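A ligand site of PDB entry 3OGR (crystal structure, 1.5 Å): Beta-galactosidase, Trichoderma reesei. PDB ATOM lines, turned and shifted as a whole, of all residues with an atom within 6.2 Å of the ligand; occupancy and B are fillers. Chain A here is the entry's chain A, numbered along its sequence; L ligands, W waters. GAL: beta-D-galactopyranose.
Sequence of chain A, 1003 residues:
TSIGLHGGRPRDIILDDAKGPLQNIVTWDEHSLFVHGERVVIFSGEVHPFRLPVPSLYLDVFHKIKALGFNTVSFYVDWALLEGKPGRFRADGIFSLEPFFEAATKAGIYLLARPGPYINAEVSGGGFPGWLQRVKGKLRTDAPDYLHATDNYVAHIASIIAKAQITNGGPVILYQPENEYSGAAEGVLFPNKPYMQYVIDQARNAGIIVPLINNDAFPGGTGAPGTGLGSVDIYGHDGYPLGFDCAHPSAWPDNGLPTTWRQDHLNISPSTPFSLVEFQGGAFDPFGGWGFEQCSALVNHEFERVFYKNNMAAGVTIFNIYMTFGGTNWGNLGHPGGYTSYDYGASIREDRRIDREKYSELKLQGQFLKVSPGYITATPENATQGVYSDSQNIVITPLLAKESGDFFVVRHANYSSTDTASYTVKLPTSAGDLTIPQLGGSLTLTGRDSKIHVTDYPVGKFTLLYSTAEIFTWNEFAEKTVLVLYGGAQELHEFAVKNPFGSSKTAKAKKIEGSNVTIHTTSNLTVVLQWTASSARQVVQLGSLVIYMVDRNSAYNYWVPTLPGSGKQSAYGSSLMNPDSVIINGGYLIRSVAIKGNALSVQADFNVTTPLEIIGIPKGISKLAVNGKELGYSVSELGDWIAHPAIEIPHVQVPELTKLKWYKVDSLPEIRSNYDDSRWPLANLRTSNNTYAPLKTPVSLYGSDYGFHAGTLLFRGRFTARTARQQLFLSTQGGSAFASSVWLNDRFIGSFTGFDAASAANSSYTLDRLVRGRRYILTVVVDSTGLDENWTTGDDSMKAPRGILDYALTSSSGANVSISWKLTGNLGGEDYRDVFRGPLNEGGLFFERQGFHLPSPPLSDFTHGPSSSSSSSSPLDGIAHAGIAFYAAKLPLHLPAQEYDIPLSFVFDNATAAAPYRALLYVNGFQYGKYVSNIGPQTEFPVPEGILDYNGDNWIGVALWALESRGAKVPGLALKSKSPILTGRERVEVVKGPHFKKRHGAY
Water W3 bridges O5 of the ligand (3.0 Å) and ND2 of Asn 120 (3.1 Å). Water W2 lies within hydrogen-bond range of OE1 of Glu 180 (2.7 Å) and O1 of the ligand (3.3 Å).
N of Ala 121 lies within hydrogen-bond range of O3 of the ligand, at 2.9 Å. OH of Tyr 344 lies within hydrogen-bond range of O6 of the ligand (2.7 Å). O of Ile 119 is in hydrogen-bond range of O3 of the ligand, 3.1 Å away. OE2 of Glu 180 is in hydrogen-bond range of O1 of the ligand, 2.7 Å away. OH of Tyr 76 sits at hydrogen-bond distance from O3 of the ligand (2.8 Å). ND2 of Asn 179 sits at hydrogen-bond distance from O2 of the ligand (2.9 Å). O4 of the ligand sits at hydrogen-bond distance from ND2 of Asn 120, at 2.8 Å. The side-chain carboxylate (OE2) of Glu 278 sits at hydrogen-bond distance from an oxygen (O2) of the ligand. The side-chain carboxylate (OE2) of Glu 122 sits at hydrogen-bond distance from an oxygen (O4) of the ligand (2.6 Å).
The side-chain carboxylate (OE2) of Glu 789 is in hydrogen-bond range of the side-chain amide nitrogen (ND2) of Asn 120 (3.3 Å). NE1 of Trp 791 is in hydrogen-bond range of OE1 of Glu 180. OH of Tyr 76 lies within hydrogen-bond range of OD1 of Asn 179, at 2.6 Å. The side-chain carboxylate (OE1) of Glu 278 lies within hydrogen-bond range of the side-chain hydroxyl (OH) of Tyr 240 (2.6 Å). OH of Tyr 342 lies within hydrogen-bond range of O of Ala 121 (3.4 Å). OE1 of Glu 122 sits at hydrogen-bond distance from OH of Tyr 342 (2.6 Å). N of Glu 180 lies within hydrogen-bond range of OD1 of Asn 215, 2.9 Å away. O of Ile 119 sits at hydrogen-bond distance from OH of Tyr 76 (3.2 Å).
Merely in contact with the ligand: Tyr 322 (3.5 Å), Phe 284 (3.5 Å), Tyr 240 (3.6 Å), Phe 244 (3.8 Å) and Tyr 342 (3.96 Å). Hydrophobic or aromatic side chains within 4 Å of the ligand: Tyr 76, Tyr 240, Phe 244, Phe 284, Tyr 322 and Tyr 344. Along chain A the residues within 4 Å of the ligand span positions 76 to 344.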
ATOM      1  N   TYR A  76      15.979   2.828   9.905  1.00  0.00           N
ATOM      2  CA  TYR A  76      16.467   1.736  10.754  1.00  0.00           C
ATOM      3  C   TYR A  76      16.271   2.025  12.217  1.00  0.00           C
ATOM      4  O   TYR A  76      16.197   3.218  12.673  1.00  0.00           O
ATOM      5  CB  TYR A  76      18.012   1.503  10.534  1.00  0.00           C
ATOM      6  CG  TYR A  76      18.369   0.803   9.234  1.00  0.00           C
ATOM      7  CD1 TYR A  76      17.708  -0.383   8.804  1.00  0.00           C
ATOM      8  CD2 TYR A  76      19.502   1.248   8.526  1.00  0.00           C
ATOM      9  CE1 TYR A  76      18.164  -1.064   7.589  1.00  0.00           C
ATOM     10  CE2 TYR A  76      19.953   0.576   7.382  1.00  0.00           C
ATOM     11  CZ  TYR A  76      19.274  -0.557   6.921  1.00  0.00           C
ATOM     12  OH  TYR A  76      19.700  -1.186   5.785  1.00  0.00           O
ATOM     13  N   ARG A 114      12.328  -0.332   9.573  1.00  0.00           N
ATOM     14  CA  ARG A 114      13.277  -1.391   9.264  1.00  0.00           C
ATOM     15  C   ARG A 114      14.090  -1.665  10.540  1.00  0.00           C
ATOM     16  O   ARG A 114      15.240  -1.196  10.702  1.00  0.00           O
ATOM     17  CB  ARG A 114      14.216  -0.959   8.071  1.00  0.00           C
ATOM     18  CG  ARG A 114      13.399  -0.267   6.918  1.00  0.00           C
ATOM     19  CD  ARG A 114      14.124  -0.281   5.598  1.00  0.00           C
ATOM     20  NE  ARG A 114      15.365   0.451   5.632  1.00  0.00           N
ATOM     21  CZ  ARG A 114      16.429   0.078   4.919  1.00  0.00           C
ATOM     22  NH1 ARG A 114      16.448  -1.097   4.203  1.00  0.00           N
ATOM     23  NH2 ARG A 114      17.519   0.884   4.882  1.00  0.00           N
ATOM     24  N   ILE A 119      20.861  -4.680  10.806  1.00  0.00           N
ATOM     25  CA  ILE A 119      20.607  -3.530   9.882  1.00  0.00           C
ATOM     26  C   ILE A 119      21.785  -3.134   8.986  1.00  0.00           C
ATOM     27  O   ILE A 119      21.587  -2.479   7.988  1.00  0.00           O
ATOM     28  CB  ILE A 119      20.081  -2.234  10.673  1.00  0.00           C
ATOM     29  CG1 ILE A 119      21.116  -1.782  11.698  1.00  0.00           C
ATOM     30  CG2 ILE A 119      18.728  -2.526  11.275  1.00  0.00           C
ATOM     31  CD1 ILE A 119      20.856  -0.333  12.148  1.00  0.00           C
ATOM     32  N   ASN A 120      22.975  -3.585   9.343  1.00  0.00           N
ATOM     33  CA  ASN A 120      24.239  -3.242   8.609  1.00  0.00           C
ATOM     34  C   ASN A 120      24.458  -1.727   8.836  1.00  0.00           C
ATOM     35  O   ASN A 120      24.892  -1.369   9.941  1.00  0.00           O
ATOM     36  CB  ASN A 120      24.188  -3.682   7.113  1.00  0.00           C
ATOM     37  CG  ASN A 120      25.551  -3.921   6.546  1.00  0.00           C
ATOM     38  OD1 ASN A 120      26.286  -4.809   7.054  1.00  0.00           O
ATOM     39  ND2 ASN A 120      25.946  -3.100   5.506  1.00  0.00           N
ATOM     40  N   ALA A 121      24.178  -0.860   7.838  1.00  0.00           N
ATOM     41  CA  ALA A 121      23.994   0.587   8.112  1.00  0.00           C
ATOM     42  C   ALA A 121      25.223   1.357   8.473  1.00  0.00           C
ATOM     43  O   ALA A 121      25.177   2.542   8.853  1.00  0.00           O
ATOM     44  CB  ALA A 121      22.886   0.860   9.187  1.00  0.00           C
ATOM     45  N   GLU A 122      26.373   0.727   8.309  1.00  0.00           N
ATOM     46  CA  GLU A 122      27.669   1.321   8.767  1.00  0.00           C
ATOM     47  C   GLU A 122      27.618   1.712  10.260  1.00  0.00           C
ATOM     48  O   GLU A 122      28.295   2.641  10.696  1.00  0.00           O
ATOM     49  CB  GLU A 122      28.088   2.536   7.902  1.00  0.00           C
ATOM     50  CG  GLU A 122      28.494   2.030   6.466  1.00  0.00           C
ATOM     51  CD  GLU A 122      27.338   1.620   5.588  1.00  0.00           C
ATOM     52  OE1 GLU A 122      26.408   2.473   5.374  1.00  0.00           O
ATOM     53  OE2 GLU A 122      27.360   0.457   5.030  1.00  0.00           O
ATOM     54  N   ASN A 179      17.706  -7.673   6.834  1.00  0.00           N
ATOM     55  CA  ASN A 179      18.294  -6.652   5.941  1.00  0.00           C
ATOM     56  C   ASN A 179      19.201  -7.349   4.927  1.00  0.00           C
ATOM     57  O   ASN A 179      20.226  -7.968   5.322  1.00  0.00           O
ATOM     58  CB  ASN A 179      19.130  -5.616   6.723  1.00  0.00           C
ATOM     59  CG  ASN A 179      19.537  -4.468   5.808  1.00  0.00           C
ATOM     60  OD1 ASN A 179      18.684  -3.607   5.496  1.00  0.00           O
ATOM     61  ND2 ASN A 179      20.780  -4.413   5.356  1.00  0.00           N
ATOM     62  N   GLU A 180      18.906  -7.208   3.640  1.00  0.00           N
ATOM     63  CA  GLU A 180      19.736  -7.814   2.594  1.00  0.00           C
ATOM     64  C   GLU A 180      20.122  -9.269   2.915  1.00  0.00           C
ATOM     65  O   GLU A 180      21.285  -9.659   2.973  1.00  0.00           O
ATOM     66  CB  GLU A 180      20.993  -6.991   2.280  1.00  0.00           C
ATOM     67  CG  GLU A 180      20.602  -5.630   1.624  1.00  0.00           C
ATOM     68  CD  GLU A 180      21.747  -5.007   0.803  1.00  0.00           C
ATOM     69  OE1 GLU A 180      22.911  -5.432   0.887  1.00  0.00           O
ATOM     70  OE2 GLU A 180      21.455  -4.024   0.038  1.00  0.00           O
ATOM     71  N   ASN A 215      14.472  -6.480   1.216  1.00  0.00           N
ATOM     72  CA  ASN A 215      15.447  -5.672   0.468  1.00  0.00           C
ATOM     73  C   ASN A 215      16.619  -6.525   0.058  1.00  0.00           C
ATOM     74  O   ASN A 215      17.713  -6.397   0.536  1.00  0.00           O
ATOM     75  CB  ASN A 215      15.891  -4.408   1.270  1.00  0.00           C
ATOM     76  CG  ASN A 215      16.725  -4.715   2.497  1.00  0.00           C
ATOM     77  OD1 ASN A 215      16.474  -5.659   3.245  1.00  0.00           O
ATOM     78  ND2 ASN A 215      17.683  -3.797   2.785  1.00  0.00           N
ATOM     79  N   ALA A 217      19.773  -7.766  -1.690  1.00  0.00           N
ATOM     80  CA  ALA A 217      20.930  -6.921  -2.129  1.00  0.00           C
ATOM     81  C   ALA A 217      21.031  -6.757  -3.621  1.00  0.00           C
ATOM     82  O   ALA A 217      21.593  -5.742  -4.117  1.00  0.00           O
ATOM     83  CB  ALA A 217      22.228  -7.566  -1.635  1.00  0.00           C
ATOM     84  N   ASP A 238      17.733  -3.784  -3.725  1.00  0.00           N
ATOM     85  CA  ASP A 238      18.502  -2.556  -3.583  1.00  0.00           C
ATOM     86  C   ASP A 238      19.404  -2.336  -4.780  1.00  0.00           C
ATOM     87  O   ASP A 238      19.502  -3.224  -5.678  1.00  0.00           O
ATOM     88  CB  ASP A 238      19.353  -2.692  -2.305  1.00  0.00           C
ATOM     89  CG  ASP A 238      18.496  -2.753  -1.036  1.00  0.00           C
ATOM     90  OD1 ASP A 238      17.294  -2.479  -1.089  1.00  0.00           O
ATOM     91  OD2 ASP A 238      19.079  -3.102   0.069  1.00  0.00           O
ATOM     92  N   TYR A 240      23.221   0.046  -5.679  1.00  0.00           N
ATOM     93  CA  TYR A 240      24.231   1.077  -5.557  1.00  0.00           C
ATOM     94  C   TYR A 240      25.134   1.023  -6.731  1.00  0.00           C
ATOM     95  O   TYR A 240      26.341   0.640  -6.619  1.00  0.00           O
ATOM     96  CB  TYR A 240      25.006   0.940  -4.227  1.00  0.00           C
ATOM     97  CG  TYR A 240      24.100   1.169  -3.026  1.00  0.00           C
ATOM     98  CD1 TYR A 240      23.313   0.122  -2.513  1.00  0.00           C
ATOM     99  CD2 TYR A 240      24.029   2.433  -2.390  1.00  0.00           C
ATOM    100  CE1 TYR A 240      22.469   0.305  -1.338  1.00  0.00           C
ATOM    101  CE2 TYR A 240      23.244   2.630  -1.258  1.00  0.00           C
ATOM    102  CZ  TYR A 240      22.458   1.585  -0.775  1.00  0.00           C
ATOM    103  OH  TYR A 240      21.695   1.782   0.352  1.00  0.00           O
ATOM    104  N   PHE A 244      31.099   2.663  -3.698  1.00  0.00           N
ATOM    105  CA  PHE A 244      31.363   3.517  -2.530  1.00  0.00           C
ATOM    106  C   PHE A 244      32.689   4.179  -2.396  1.00  0.00           C
ATOM    107  O   PHE A 244      33.006   4.846  -1.349  1.00  0.00           O
ATOM    108  CB  PHE A 244      31.020   2.733  -1.260  1.00  0.00           C
ATOM    109  CG  PHE A 244      29.665   2.141  -1.283  1.00  0.00           C
ATOM    110  CD1 PHE A 244      29.494   0.794  -1.595  1.00  0.00           C
ATOM    111  CD2 PHE A 244      28.524   2.932  -1.030  1.00  0.00           C
ATOM    112  CE1 PHE A 244      28.236   0.197  -1.549  1.00  0.00           C
ATOM    113  CE2 PHE A 244      27.267   2.369  -1.052  1.00  0.00           C
ATOM    114  CZ  PHE A 244      27.092   1.011  -1.287  1.00  0.00           C
ATOM    115  N   GLU A 278      16.287   0.283  -1.226  1.00  0.00           N
ATOM    116  CA  GLU A 278      17.437   1.223  -1.059  1.00  0.00           C
ATOM    117  C   GLU A 278      18.019   1.476  -2.428  1.00  0.00           C
ATOM    118  O   GLU A 278      18.464   0.520  -3.098  1.00  0.00           O
ATOM    119  CB  GLU A 278      18.559   0.602  -0.213  1.00  0.00           C
ATOM    120  CG  GLU A 278      18.135   0.252   1.255  1.00  0.00           C
ATOM    121  CD  GLU A 278      19.258  -0.427   1.970  1.00  0.00           C
ATOM    122  OE1 GLU A 278      20.435  -0.178   1.592  1.00  0.00           O
ATOM    123  OE2 GLU A 278      18.979  -1.190   2.887  1.00  0.00           O
ATOM    124  N   ALA A 283      27.301   7.901  -0.697  1.00  0.00           N
ATOM    125  CA  ALA A 283      28.250   6.789  -0.411  1.00  0.00           C
ATOM    126  C   ALA A 283      28.667   6.925   1.018  1.00  0.00           C
ATOM    127  O   ALA A 283      28.772   8.087   1.506  1.00  0.00           O
ATOM    128  CB  ALA A 283      29.445   6.804  -1.371  1.00  0.00           C
ATOM    129  N   PHE A 284      29.044   5.823   1.639  1.00  0.00           N
ATOM    130  CA  PHE A 284      29.796   5.924   2.895  1.00  0.00           C
ATOM    131  C   PHE A 284      31.260   6.205   2.556  1.00  0.00           C
ATOM    132  O   PHE A 284      31.675   6.205   1.366  1.00  0.00           O
ATOM    133  CB  PHE A 284      29.665   4.618   3.730  1.00  0.00           C
ATOM    134  CG  PHE A 284      30.069   3.363   3.005  1.00  0.00           C
ATOM    135  CD1 PHE A 284      31.448   3.119   2.713  1.00  0.00           C
ATOM    136  CD2 PHE A 284      29.117   2.470   2.579  1.00  0.00           C
ATOM    137  CE1 PHE A 284      31.851   1.904   2.058  1.00  0.00           C
ATOM    138  CE2 PHE A 284      29.484   1.263   1.925  1.00  0.00           C
ATOM    139  CZ  PHE A 284      30.821   0.979   1.685  1.00  0.00           C
ATOM    140  N   TYR A 322      18.727   6.039  -0.233  1.00  0.00           N
ATOM    141  CA  TYR A 322      19.559   5.807   0.929  1.00  0.00           C
ATOM    142  C   TYR A 322      20.931   6.473   0.691  1.00  0.00           C
ATOM    143  O   TYR A 322      21.581   6.056  -0.261  1.00  0.00           O
ATOM    144  CB  TYR A 322      19.735   4.267   1.107  1.00  0.00           C
ATOM    145  CG  TYR A 322      20.523   3.900   2.353  1.00  0.00           C
ATOM    146  CD1 TYR A 322      21.893   4.156   2.476  1.00  0.00           C
ATOM    147  CD2 TYR A 322      19.879   3.255   3.455  1.00  0.00           C
ATOM    148  CE1 TYR A 322      22.588   3.860   3.629  1.00  0.00           C
ATOM    149  CE2 TYR A 322      20.581   2.946   4.633  1.00  0.00           C
ATOM    150  CZ  TYR A 322      21.920   3.264   4.722  1.00  0.00           C
ATOM    151  OH  TYR A 322      22.575   2.987   5.917  1.00  0.00           O
ATOM    152  N   TYR A 342      28.393  10.942   9.170  1.00  0.00           N
ATOM    153  CA  TYR A 342      27.646  10.081   8.210  1.00  0.00           C
ATOM    154  C   TYR A 342      26.880  11.027   7.242  1.00  0.00           C
ATOM    155  O   TYR A 342      25.757  10.771   6.833  1.00  0.00           O
ATOM    156  CB  TYR A 342      26.654   9.157   8.958  1.00  0.00           C
ATOM    157  CG  TYR A 342      26.228   7.979   8.084  1.00  0.00           C
ATOM    158  CD1 TYR A 342      27.146   7.070   7.613  1.00  0.00           C
ATOM    159  CD2 TYR A 342      24.819   7.717   7.914  1.00  0.00           C
ATOM    160  CE1 TYR A 342      26.753   5.869   6.910  1.00  0.00           C
ATOM    161  CE2 TYR A 342      24.444   6.558   7.209  1.00  0.00           C
ATOM    162  CZ  TYR A 342      25.384   5.656   6.717  1.00  0.00           C
ATOM    163  OH  TYR A 342      24.944   4.517   6.103  1.00  0.00           O
ATOM    164  N   TYR A 344      27.296  11.311   4.195  1.00  0.00           N
ATOM    165  CA  TYR A 344      26.965  10.360   3.105  1.00  0.00           C
ATOM    166  C   TYR A 344      26.946  11.049   1.732  1.00  0.00           C
ATOM    167  O   TYR A 344      26.661  10.393   0.722  1.00  0.00           O
ATOM    168  CB  TYR A 344      25.554   9.716   3.356  1.00  0.00           C
ATOM    169  CG  TYR A 344      25.418   8.323   2.795  1.00  0.00           C
ATOM    170  CD1 TYR A 344      25.939   7.244   3.460  1.00  0.00           C
ATOM    171  CD2 TYR A 344      24.793   8.109   1.589  1.00  0.00           C
ATOM    172  CE1 TYR A 344      25.813   5.940   2.957  1.00  0.00           C
ATOM    173  CE2 TYR A 344      24.641   6.805   1.054  1.00  0.00           C
ATOM    174  CZ  TYR A 344      25.211   5.733   1.729  1.00  0.00           C
ATOM    175  OH  TYR A 344      25.121   4.442   1.189  1.00  0.00           O
ATOM    176  N   GLU A 789      30.647  -5.057  10.959  1.00  0.00           N
ATOM    177  CA  GLU A 789      29.392  -5.591  10.444  1.00  0.00           C
ATOM    178  C   GLU A 789      29.430  -7.110  10.213  1.00  0.00           C
ATOM    179  O   GLU A 789      30.472  -7.755  10.396  1.00  0.00           O
ATOM    180  CB  GLU A 789      29.068  -4.875   9.138  1.00  0.00           C
ATOM    181  CG  GLU A 789      28.679  -3.413   9.367  1.00  0.00           C
ATOM    182  CD  GLU A 789      28.545  -2.682   8.067  1.00  0.00           C
ATOM    183  OE1 GLU A 789      29.375  -2.908   7.153  1.00  0.00           O
ATOM    184  OE2 GLU A 789      27.649  -1.815   7.970  1.00  0.00           O
ATOM    185  N   TRP A 791      27.777  -8.741   7.274  1.00  0.00           N
ATOM    186  CA  TRP A 791      26.938  -8.665   6.116  1.00  0.00           C
ATOM    187  C   TRP A 791      26.772 -10.016   5.416  1.00  0.00           C
ATOM    188  O   TRP A 791      25.822 -10.152   4.608  1.00  0.00           O
ATOM    189  CB  TRP A 791      27.440  -7.570   5.137  1.00  0.00           C
ATOM    190  CG  TRP A 791      26.527  -7.385   3.980  1.00  0.00           C
ATOM    191  CD1 TRP A 791      25.587  -6.429   3.876  1.00  0.00           C
ATOM    192  CD2 TRP A 791      26.516  -8.126   2.702  1.00  0.00           C
ATOM    193  NE1 TRP A 791      24.925  -6.526   2.650  1.00  0.00           N
ATOM    194  CE2 TRP A 791      25.459  -7.567   1.915  1.00  0.00           C
ATOM    195  CE3 TRP A 791      27.258  -9.257   2.187  1.00  0.00           C
ATOM    196  CZ2 TRP A 791      25.115  -8.064   0.628  1.00  0.00           C
ATOM    197  CZ3 TRP A 791      26.916  -9.771   0.875  1.00  0.00           C
ATOM    198  CH2 TRP A 791      25.845  -9.161   0.125  1.00  0.00           C
HETATM  199  C1  GAL L   1      23.160  -1.520   1.796  1.00  0.00           C
HETATM  200  C2  GAL L   1      22.794  -1.884   3.274  1.00  0.00           C
HETATM  201  C3  GAL L   1      22.716  -0.633   4.126  1.00  0.00           C
HETATM  202  C4  GAL L   1      24.026   0.165   4.007  1.00  0.00           C
HETATM  203  C5  GAL L   1      24.287   0.429   2.533  1.00  0.00           C
HETATM  204  C6  GAL L   1      25.642   1.099   2.240  1.00  0.00           C
HETATM  205  O1  GAL L   1      23.591  -2.665   1.051  1.00  0.00           O
HETATM  206  O2  GAL L   1      21.504  -2.497   3.270  1.00  0.00           O
HETATM  207  O3  GAL L   1      22.513  -0.988   5.483  1.00  0.00           O
HETATM  208  O4  GAL L   1      25.059  -0.652   4.546  1.00  0.00           O
HETATM  209  O5  GAL L   1      24.370  -0.826   1.815  1.00  0.00           O
HETATM  210  O6  GAL L   1      25.642   2.397   2.829  1.00  0.00           O
HETATM  211  O   HOH W   1      25.781  -2.240  -0.635  1.00  0.00           O
HETATM  212  O   HOH W   2      25.028  -5.012  -0.761  1.00  0.00           O
HETATM  213  O   HOH W   3      26.688  -2.533   2.529  1.00  0.00           O
